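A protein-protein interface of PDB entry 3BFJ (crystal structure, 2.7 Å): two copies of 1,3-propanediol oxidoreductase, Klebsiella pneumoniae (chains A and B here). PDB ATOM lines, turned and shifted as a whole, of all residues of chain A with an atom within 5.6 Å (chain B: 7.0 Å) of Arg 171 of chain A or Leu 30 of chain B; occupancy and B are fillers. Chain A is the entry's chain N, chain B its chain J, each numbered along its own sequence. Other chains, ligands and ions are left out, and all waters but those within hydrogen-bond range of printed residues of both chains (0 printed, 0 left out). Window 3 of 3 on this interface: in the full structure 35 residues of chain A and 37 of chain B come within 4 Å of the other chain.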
ATOM      1  N   HIS A 117     -13.210  34.631 -15.268  1.00  0.00           N
ATOM      2  CA  HIS A 117     -12.285  34.481 -14.150  1.00  0.00           C
ATOM      3  C   HIS A 117     -10.926  35.124 -14.439  1.00  0.00           C
ATOM      4  O   HIS A 117     -10.359  34.918 -15.517  1.00  0.00           O
ATOM      5  CB  HIS A 117     -12.133  33.002 -13.784  1.00  0.00           C
ATOM      6  CG  HIS A 117     -13.398  32.370 -13.283  1.00  0.00           C
ATOM      7  ND1 HIS A 117     -14.347  31.834 -14.127  1.00  0.00           N
ATOM      8  CD2 HIS A 117     -13.871  32.195 -12.027  1.00  0.00           C
ATOM      9  CE1 HIS A 117     -15.349  31.354 -13.412  1.00  0.00           C
ATOM     10  NE2 HIS A 117     -15.085  31.559 -12.134  1.00  0.00           N
ATOM     11  N   GLU A 128     -12.961  21.905  -7.952  1.00  0.00           N
ATOM     12  CA  GLU A 128     -13.917  23.007  -7.886  1.00  0.00           C
ATOM     13  C   GLU A 128     -13.234  24.318  -7.483  1.00  0.00           C
ATOM     14  O   GLU A 128     -13.141  24.656  -6.299  1.00  0.00           O
ATOM     15  CB  GLU A 128     -15.050  22.648  -6.924  1.00  0.00           C
ATOM     16  CG  GLU A 128     -16.298  23.489  -7.087  1.00  0.00           C
ATOM     17  CD  GLU A 128     -17.563  22.688  -6.841  1.00  0.00           C
ATOM     18  OE1 GLU A 128     -18.218  22.925  -5.800  1.00  0.00           O
ATOM     19  OE2 GLU A 128     -17.891  21.817  -7.685  1.00  0.00           O
ATOM     20  N   LEU A 130     -13.821  27.258  -9.513  1.00  0.00           N
ATOM     21  CA  LEU A 130     -14.597  28.316 -10.163  1.00  0.00           C
ATOM     22  C   LEU A 130     -15.590  28.964  -9.202  1.00  0.00           C
ATOM     23  O   LEU A 130     -16.296  28.270  -8.461  1.00  0.00           O
ATOM     24  CB  LEU A 130     -15.319  27.768 -11.398  1.00  0.00           C
ATOM     25  CG  LEU A 130     -14.587  27.808 -12.747  1.00  0.00           C
ATOM     26  CD1 LEU A 130     -13.202  27.170 -12.705  1.00  0.00           C
ATOM     27  CD2 LEU A 130     -15.435  27.156 -13.826  1.00  0.00           C
ATOM     28  N   THR A 131     -15.636  30.295  -9.227  1.00  0.00           N
ATOM     29  CA  THR A 131     -16.471  31.068  -8.307  1.00  0.00           C
ATOM     30  C   THR A 131     -17.719  31.622  -8.995  1.00  0.00           C
ATOM     31  O   THR A 131     -18.775  31.744  -8.371  1.00  0.00           O
ATOM     32  CB  THR A 131     -15.685  32.247  -7.693  1.00  0.00           C
ATOM     33  OG1 THR A 131     -14.320  31.864  -7.494  1.00  0.00           O
ATOM     34  CG2 THR A 131     -16.294  32.676  -6.358  1.00  0.00           C
ATOM     35  N   ASN A 132     -17.588  31.945 -10.279  1.00  0.00           N
ATOM     36  CA  ASN A 132     -18.618  32.684 -11.013  1.00  0.00           C
ATOM     37  C   ASN A 132     -19.196  31.894 -12.188  1.00  0.00           C
ATOM     38  O   ASN A 132     -18.475  31.111 -12.814  1.00  0.00           O
ATOM     39  CB  ASN A 132     -18.043  34.011 -11.514  1.00  0.00           C
ATOM     40  CG  ASN A 132     -17.123  34.664 -10.506  1.00  0.00           C
ATOM     41  OD1 ASN A 132     -17.525  34.963  -9.381  1.00  0.00           O
ATOM     42  ND2 ASN A 132     -15.875  34.886 -10.905  1.00  0.00           N
ATOM     43  N   PRO A 133     -20.494  32.108 -12.502  1.00  0.00           N
ATOM     44  CA  PRO A 133     -21.122  31.386 -13.617  1.00  0.00           C
ATOM     45  C   PRO A 133     -20.506  31.774 -14.957  1.00  0.00           C
ATOM     46  O   PRO A 133     -20.157  32.940 -15.164  1.00  0.00           O
ATOM     47  CB  PRO A 133     -22.586  31.841 -13.557  1.00  0.00           C
ATOM     48  CG  PRO A 133     -22.550  33.157 -12.846  1.00  0.00           C
ATOM     49  CD  PRO A 133     -21.438  33.036 -11.848  1.00  0.00           C
ATOM     50  N   LEU A 134     -20.364  30.799 -15.848  1.00  0.00           N
ATOM     51  CA  LEU A 134     -19.828  31.042 -17.184  1.00  0.00           C
ATOM     52  C   LEU A 134     -20.884  31.710 -18.067  1.00  0.00           C
ATOM     53  O   LEU A 134     -22.055  31.775 -17.683  1.00  0.00           O
ATOM     54  CB  LEU A 134     -19.362  29.728 -17.826  1.00  0.00           C
ATOM     55  CG  LEU A 134     -18.308  28.831 -17.164  1.00  0.00           C
ATOM     56  CD1 LEU A 134     -17.643  27.964 -18.226  1.00  0.00           C
ATOM     57  CD2 LEU A 134     -17.253  29.617 -16.387  1.00  0.00           C
ATOM     58  N   SER A 169     -15.372  21.399 -12.763  1.00  0.00           N
ATOM     59  CA  SER A 169     -16.379  22.223 -12.097  1.00  0.00           C
ATOM     60  C   SER A 169     -17.790  21.951 -12.599  1.00  0.00           C
ATOM     61  O   SER A 169     -17.995  21.635 -13.772  1.00  0.00           O
ATOM     62  CB  SER A 169     -16.054  23.708 -12.266  1.00  0.00           C
ATOM     63  OG  SER A 169     -16.822  24.507 -11.386  1.00  0.00           O
ATOM     64  N   TRP A 170     -18.763  22.095 -11.702  1.00  0.00           N
ATOM     65  CA  TRP A 170     -20.172  22.007 -12.071  1.00  0.00           C
ATOM     66  C   TRP A 170     -20.579  23.173 -12.984  1.00  0.00           C
ATOM     67  O   TRP A 170     -21.649  23.155 -13.600  1.00  0.00           O
ATOM     68  CB  TRP A 170     -21.048  21.970 -10.814  1.00  0.00           C
ATOM     69  CG  TRP A 170     -21.112  23.273 -10.098  1.00  0.00           C
ATOM     70  CD1 TRP A 170     -20.169  23.797  -9.264  1.00  0.00           C
ATOM     71  CD2 TRP A 170     -22.176  24.230 -10.158  1.00  0.00           C
ATOM     72  NE1 TRP A 170     -20.579  25.020  -8.797  1.00  0.00           N
ATOM     73  CE2 TRP A 170     -21.807  25.314  -9.333  1.00  0.00           C
ATOM     74  CE3 TRP A 170     -23.403  24.278 -10.834  1.00  0.00           C
ATOM     75  CZ2 TRP A 170     -22.625  26.438  -9.157  1.00  0.00           C
ATOM     76  CZ3 TRP A 170     -24.217  25.396 -10.664  1.00  0.00           C
ATOM     77  CH2 TRP A 170     -23.822  26.462  -9.829  1.00  0.00           C
ATOM     78  N   ARG A 171     -19.720  24.183 -13.062  1.00  0.00           N
ATOM     79  CA  ARG A 171     -19.966  25.342 -13.903  1.00  0.00           C
ATOM     80  C   ARG A 171     -19.466  25.127 -15.327  1.00  0.00           C
ATOM     81  O   ARG A 171     -19.797  25.902 -16.223  1.00  0.00           O
ATOM     82  CB  ARG A 171     -19.339  26.594 -13.285  1.00  0.00           C
ATOM     83  CG  ARG A 171     -19.935  26.961 -11.941  1.00  0.00           C
ATOM     84  CD  ARG A 171     -19.583  28.369 -11.577  1.00  0.00           C
ATOM     85  NE  ARG A 171     -20.064  28.760 -10.252  1.00  0.00           N
ATOM     86  CZ  ARG A 171     -21.264  29.282 -10.006  1.00  0.00           C
ATOM     87  NH1 ARG A 171     -22.141  29.459 -10.991  1.00  0.00           N
ATOM     88  NH2 ARG A 171     -21.594  29.614  -8.764  1.00  0.00           N
ATOM     89  N   ASN A 172     -18.674  24.075 -15.530  1.00  0.00           N
ATOM     90  CA  ASN A 172     -18.190  23.707 -16.865  1.00  0.00           C
ATOM     91  C   ASN A 172     -19.265  23.023 -17.702  1.00  0.00           C
ATOM     92  O   ASN A 172     -19.171  22.983 -18.933  1.00  0.00           O
ATOM     93  CB  ASN A 172     -16.967  22.794 -16.768  1.00  0.00           C
ATOM     94  CG  ASN A 172     -15.705  23.534 -16.382  1.00  0.00           C
ATOM     95  OD1 ASN A 172     -14.699  22.918 -16.042  1.00  0.00           O
ATOM     96  ND2 ASN A 172     -15.748  24.860 -16.434  1.00  0.00           N
ATOM     97  N   LEU A 173     -20.269  22.480 -17.012  1.00  0.00           N
ATOM     98  CA  LEU A 173     -21.431  21.847 -17.622  1.00  0.00           C
ATOM     99  C   LEU A 173     -22.146  22.782 -18.579  1.00  0.00           C
ATOM    100  O   LEU A 173     -22.678  23.807 -18.150  1.00  0.00           O
ATOM    101  CB  LEU A 173     -22.410  21.433 -16.526  1.00  0.00           C
ATOM    102  CG  LEU A 173     -22.645  19.974 -16.132  1.00  0.00           C
ATOM    103  CD1 LEU A 173     -21.424  19.082 -16.320  1.00  0.00           C
ATOM    104  CD2 LEU A 173     -23.135  19.938 -14.694  1.00  0.00           C
ATOM    105  N   PRO A 174     -22.163  22.443 -19.880  1.00  0.00           N
ATOM    106  CA  PRO A 174     -22.944  23.225 -20.842  1.00  0.00           C
ATOM    107  C   PRO A 174     -24.383  23.469 -20.382  1.00  0.00           C
ATOM    108  O   PRO A 174     -24.924  22.714 -19.576  1.00  0.00           O
ATOM    109  CB  PRO A 174     -22.929  22.349 -22.098  1.00  0.00           C
ATOM    110  CG  PRO A 174     -21.646  21.596 -21.998  1.00  0.00           C
ATOM    111  CD  PRO A 174     -21.439  21.335 -20.530  1.00  0.00           C
ATOM    112  N   ASN B  12     -29.286  20.156 -12.775  1.00  0.00           N
ATOM    113  CA  ASN B  12     -27.859  20.376 -13.002  1.00  0.00           C
ATOM    114  C   ASN B  12     -26.969  19.477 -12.145  1.00  0.00           C
ATOM    115  O   ASN B  12     -26.080  18.784 -12.649  1.00  0.00           O
ATOM    116  CB  ASN B  12     -27.546  21.844 -12.681  1.00  0.00           C
ATOM    117  CG  ASN B  12     -26.528  22.452 -13.616  1.00  0.00           C
ATOM    118  OD1 ASN B  12     -26.096  21.825 -14.582  1.00  0.00           O
ATOM    119  ND2 ASN B  12     -26.145  23.695 -13.338  1.00  0.00           N
ATOM    120  N   VAL B  13     -27.234  19.499 -10.844  1.00  0.00           N
ATOM    121  CA  VAL B  13     -26.400  18.841  -9.852  1.00  0.00           C
ATOM    122  C   VAL B  13     -27.293  17.976  -8.965  1.00  0.00           C
ATOM    123  O   VAL B  13     -28.310  18.448  -8.447  1.00  0.00           O
ATOM    124  CB  VAL B  13     -25.616  19.893  -9.008  1.00  0.00           C
ATOM    125  CG1 VAL B  13     -24.903  19.247  -7.846  1.00  0.00           C
ATOM    126  CG2 VAL B  13     -24.613  20.630  -9.872  1.00  0.00           C
ATOM    127  N   PHE B  15     -27.387  14.852  -5.774  1.00  0.00           N
ATOM    128  CA  PHE B  15     -26.685  14.148  -4.697  1.00  0.00           C
ATOM    129  C   PHE B  15     -27.482  12.955  -4.166  1.00  0.00           C
ATOM    130  O   PHE B  15     -28.671  13.077  -3.867  1.00  0.00           O
ATOM    131  CB  PHE B  15     -26.367  15.102  -3.543  1.00  0.00           C
ATOM    132  CG  PHE B  15     -25.244  16.053  -3.829  1.00  0.00           C
ATOM    133  CD1 PHE B  15     -25.505  17.335  -4.310  1.00  0.00           C
ATOM    134  CD2 PHE B  15     -23.921  15.675  -3.605  1.00  0.00           C
ATOM    135  CE1 PHE B  15     -24.467  18.221  -4.572  1.00  0.00           C
ATOM    136  CE2 PHE B  15     -22.871  16.557  -3.865  1.00  0.00           C
ATOM    137  CZ  PHE B  15     -23.147  17.831  -4.353  1.00  0.00           C
ATOM    138  N   VAL B  23     -24.695  18.293   2.428  1.00  0.00           N
ATOM    139  CA  VAL B  23     -24.320  19.278   1.404  1.00  0.00           C
ATOM    140  C   VAL B  23     -25.302  20.453   1.234  1.00  0.00           C
ATOM    141  O   VAL B  23     -24.957  21.442   0.581  1.00  0.00           O
ATOM    142  CB  VAL B  23     -24.000  18.633   0.014  1.00  0.00           C
ATOM    143  CG1 VAL B  23     -22.796  17.702   0.109  1.00  0.00           C
ATOM    144  CG2 VAL B  23     -25.210  17.915  -0.564  1.00  0.00           C
ATOM    145  N   GLY B  25     -26.355  23.032   2.991  1.00  0.00           N
ATOM    146  CA  GLY B  25     -25.789  24.336   3.312  1.00  0.00           C
ATOM    147  C   GLY B  25     -24.729  24.789   2.324  1.00  0.00           C
ATOM    148  O   GLY B  25     -24.766  25.925   1.849  1.00  0.00           O
ATOM    149  N   GLU B  26     -23.791  23.893   2.009  1.00  0.00           N
ATOM    150  CA  GLU B  26     -22.677  24.190   1.096  1.00  0.00           C
ATOM    151  C   GLU B  26     -23.155  24.558  -0.306  1.00  0.00           C
ATOM    152  O   GLU B  26     -22.600  25.456  -0.940  1.00  0.00           O
ATOM    153  CB  GLU B  26     -21.704  23.003   1.016  1.00  0.00           C
ATOM    154  CG  GLU B  26     -20.387  23.326   0.305  1.00  0.00           C
ATOM    155  CD  GLU B  26     -19.499  22.107   0.107  1.00  0.00           C
ATOM    156  OE1 GLU B  26     -18.919  21.615   1.106  1.00  0.00           O
ATOM    157  OE2 GLU B  26     -19.369  21.656  -1.054  1.00  0.00           O
ATOM    158  N   ARG B  27     -24.187  23.862  -0.776  1.00  0.00           N
ATOM    159  CA  ARG B  27     -24.710  24.067  -2.124  1.00  0.00           C
ATOM    160  C   ARG B  27     -25.574  25.321  -2.246  1.00  0.00           C
ATOM    161  O   ARG B  27     -25.919  25.734  -3.354  1.00  0.00           O
ATOM    162  CB  ARG B  27     -25.451  22.818  -2.619  1.00  0.00           C
ATOM    163  CG  ARG B  27     -24.526  21.740  -3.154  1.00  0.00           C
ATOM    164  CD  ARG B  27     -23.975  22.141  -4.512  1.00  0.00           C
ATOM    165  NE  ARG B  27     -22.742  21.435  -4.850  1.00  0.00           N
ATOM    166  CZ  ARG B  27     -22.086  21.581  -6.000  1.00  0.00           C
ATOM    167  NH1 ARG B  27     -22.545  22.412  -6.930  1.00  0.00           N
ATOM    168  NH2 ARG B  27     -20.966  20.900  -6.220  1.00  0.00           N
ATOM    169  N   CYS B  28     -25.912  25.925  -1.110  1.00  0.00           N
ATOM    170  CA  CYS B  28     -26.581  27.223  -1.095  1.00  0.00           C
ATOM    171  C   CYS B  28     -25.565  28.350  -1.271  1.00  0.00           C
ATOM    172  O   CYS B  28     -25.831  29.335  -1.966  1.00  0.00           O
ATOM    173  CB  CYS B  28     -27.369  27.411   0.202  1.00  0.00           C
ATOM    174  SG  CYS B  28     -28.860  26.407   0.308  1.00  0.00           S
ATOM    175  N   GLN B  29     -24.404  28.192  -0.633  1.00  0.00           N
ATOM    176  CA  GLN B  29     -23.284  29.125  -0.775  1.00  0.00           C
ATOM    177  C   GLN B  29     -22.825  29.231  -2.226  1.00  0.00           C
ATOM    178  O   GLN B  29     -22.453  30.310  -2.691  1.00  0.00           O
ATOM    179  CB  GLN B  29     -22.105  28.682   0.092  1.00  0.00           C
ATOM    180  CG  GLN B  29     -22.274  28.946   1.579  1.00  0.00           C
ATOM    181  CD  GLN B  29     -21.136  28.371   2.410  1.00  0.00           C
ATOM    182  OE1 GLN B  29     -20.745  28.948   3.427  1.00  0.00           O
ATOM    183  NE2 GLN B  29     -20.599  27.230   1.980  1.00  0.00           N
ATOM    184  N   LEU B  30     -22.855  28.101  -2.929  1.00  0.00           N
ATOM    185  CA  LEU B  30     -22.414  28.033  -4.315  1.00  0.00           C
ATOM    186  C   LEU B  30     -23.442  28.635  -5.265  1.00  0.00           C
ATOM    187  O   LEU B  30     -23.082  29.197  -6.299  1.00  0.00           O
ATOM    188  CB  LEU B  30     -22.095  26.585  -4.704  1.00  0.00           C
ATOM    189  CG  LEU B  30     -20.905  25.934  -3.988  1.00  0.00           C
ATOM    190  CD1 LEU B  30     -20.918  24.435  -4.204  1.00  0.00           C
ATOM    191  CD2 LEU B  30     -19.574  26.534  -4.438  1.00  0.00           C
ATOM    192  N   LEU B  31     -24.718  28.520  -4.907  1.00  0.00           N
ATOM    193  CA  LEU B  31     -25.798  29.067  -5.726  1.00  0.00           C
ATOM    194  C   LEU B  31     -25.961  30.568  -5.545  1.00  0.00           C
ATOM    195  O   LEU B  31     -26.478  31.249  -6.430  1.00  0.00           O
ATOM    196  CB  LEU B  31     -27.119  28.344  -5.447  1.00  0.00           C
ATOM    197  CG  LEU B  31     -27.289  26.982  -6.129  1.00  0.00           C
ATOM    198  CD1 LEU B  31     -28.444  26.210  -5.518  1.00  0.00           C
ATOM    199  CD2 LEU B  31     -27.476  27.126  -7.639  1.00  0.00           C
ATOM    200  N   GLY B  32     -25.517  31.077  -4.398  1.00  0.00           N
ATOM    201  CA  GLY B  32     -25.587  32.506  -4.107  1.00  0.00           C
ATOM    202  C   GLY B  32     -26.650  32.864  -3.086  1.00  0.00           C
ATOM    203  O   GLY B  32     -26.910  34.048  -2.846  1.00  0.00           O
ATOM    204  N   GLY B  33     -27.250  31.844  -2.478  1.00  0.00           N
ATOM    205  CA  GLY B  33     -28.336  32.028  -1.515  1.00  0.00           C
ATOM    206  C   GLY B  33     -27.889  32.466  -0.131  1.00  0.00           C
ATOM    207  O   GLY B  33     -27.135  31.760   0.544  1.00  0.00           O
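Arg 171 of chain A touches just one residue of chain B: Leu 30 (2.9 Å). Of the printed residues of chain A, Leu 30 of chain B touches Glu 128, Trp 170 and Arg 171. Of the printed residues of chain A, Asn 12 of chain B touches Trp 170 and Leu 173. Of the printed residues of chain B, Leu 173 of chain A touches Asn 12. Of the printed residues of chain A, Val 13 of chain B touches Trp 170. Of the printed residues of chain B, Trp 170 of chain A touches Asn 12 (3.7 Å), Val 13 (3.9 Å), Arg 27 (3.6 Å) and Leu 30 (3.999 Å). Printed residues of chain A within 4 Å of Arg 27 of chain B: Glu 128 (3.4 Å) and Trp 170 (3.6 Å). Gln 29 of chain B touches none of the printed residues of chain A.
Among the printed residues, merely in contact across the chains: Glu 128 of chain A with Leu 30 of chain B (3.5 Å), Leu 173 of chain A with Asn 12 of chain B (3.5 Å), Trp 170 of chain A with Arg 27 of chain B (3.6 Å), Trp 170 of chain A with Asn 12 of chain B (3.7 Å), Trp 170 of chain A with Val 13 of chain B (3.9 Å) and Trp 170 of chain A with Leu 30 of chain B (3.999 Å).
OE1 of Glu 128 of chain A lies within salt-bridge range of NH2 of Arg 27 of chain B, 3.4 Å away. The guanidinium group (NH2) of Arg 171 of chain A sits at hydrogen-bond distance from the backbone carbonyl oxygen (O) of Leu 30 of chain B.
OG of Ser 169 of chain A sits close to N of Arg 171 of chain A (3.4 Å).
Of the 13 printed residues of chain A, 4 touch a printed residue of chain B. Printed residues of chain A that touch a printed residue of chain B: Glu 128, Trp 170, Arg 171 and Leu 173. Hydrophobic or aromatic side chains of chain A that line the printed part of chain B: Trp 170 and Leu 173. Of the 13 printed residues of chain B, 4 touch a printed residue of chain A. Hydrophobic or aromatic side chains of chain B within 4 Å of the printed part of chain A: Val 13 and Leu 30. Among the printed residues, Asp or Glu carboxylates within 4 Å of a Lys or Arg side-chain nitrogen of the other chain: Glu 128 of chain A with Arg 27 of chain B (3.4 Å).
No position is printed for both chains.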
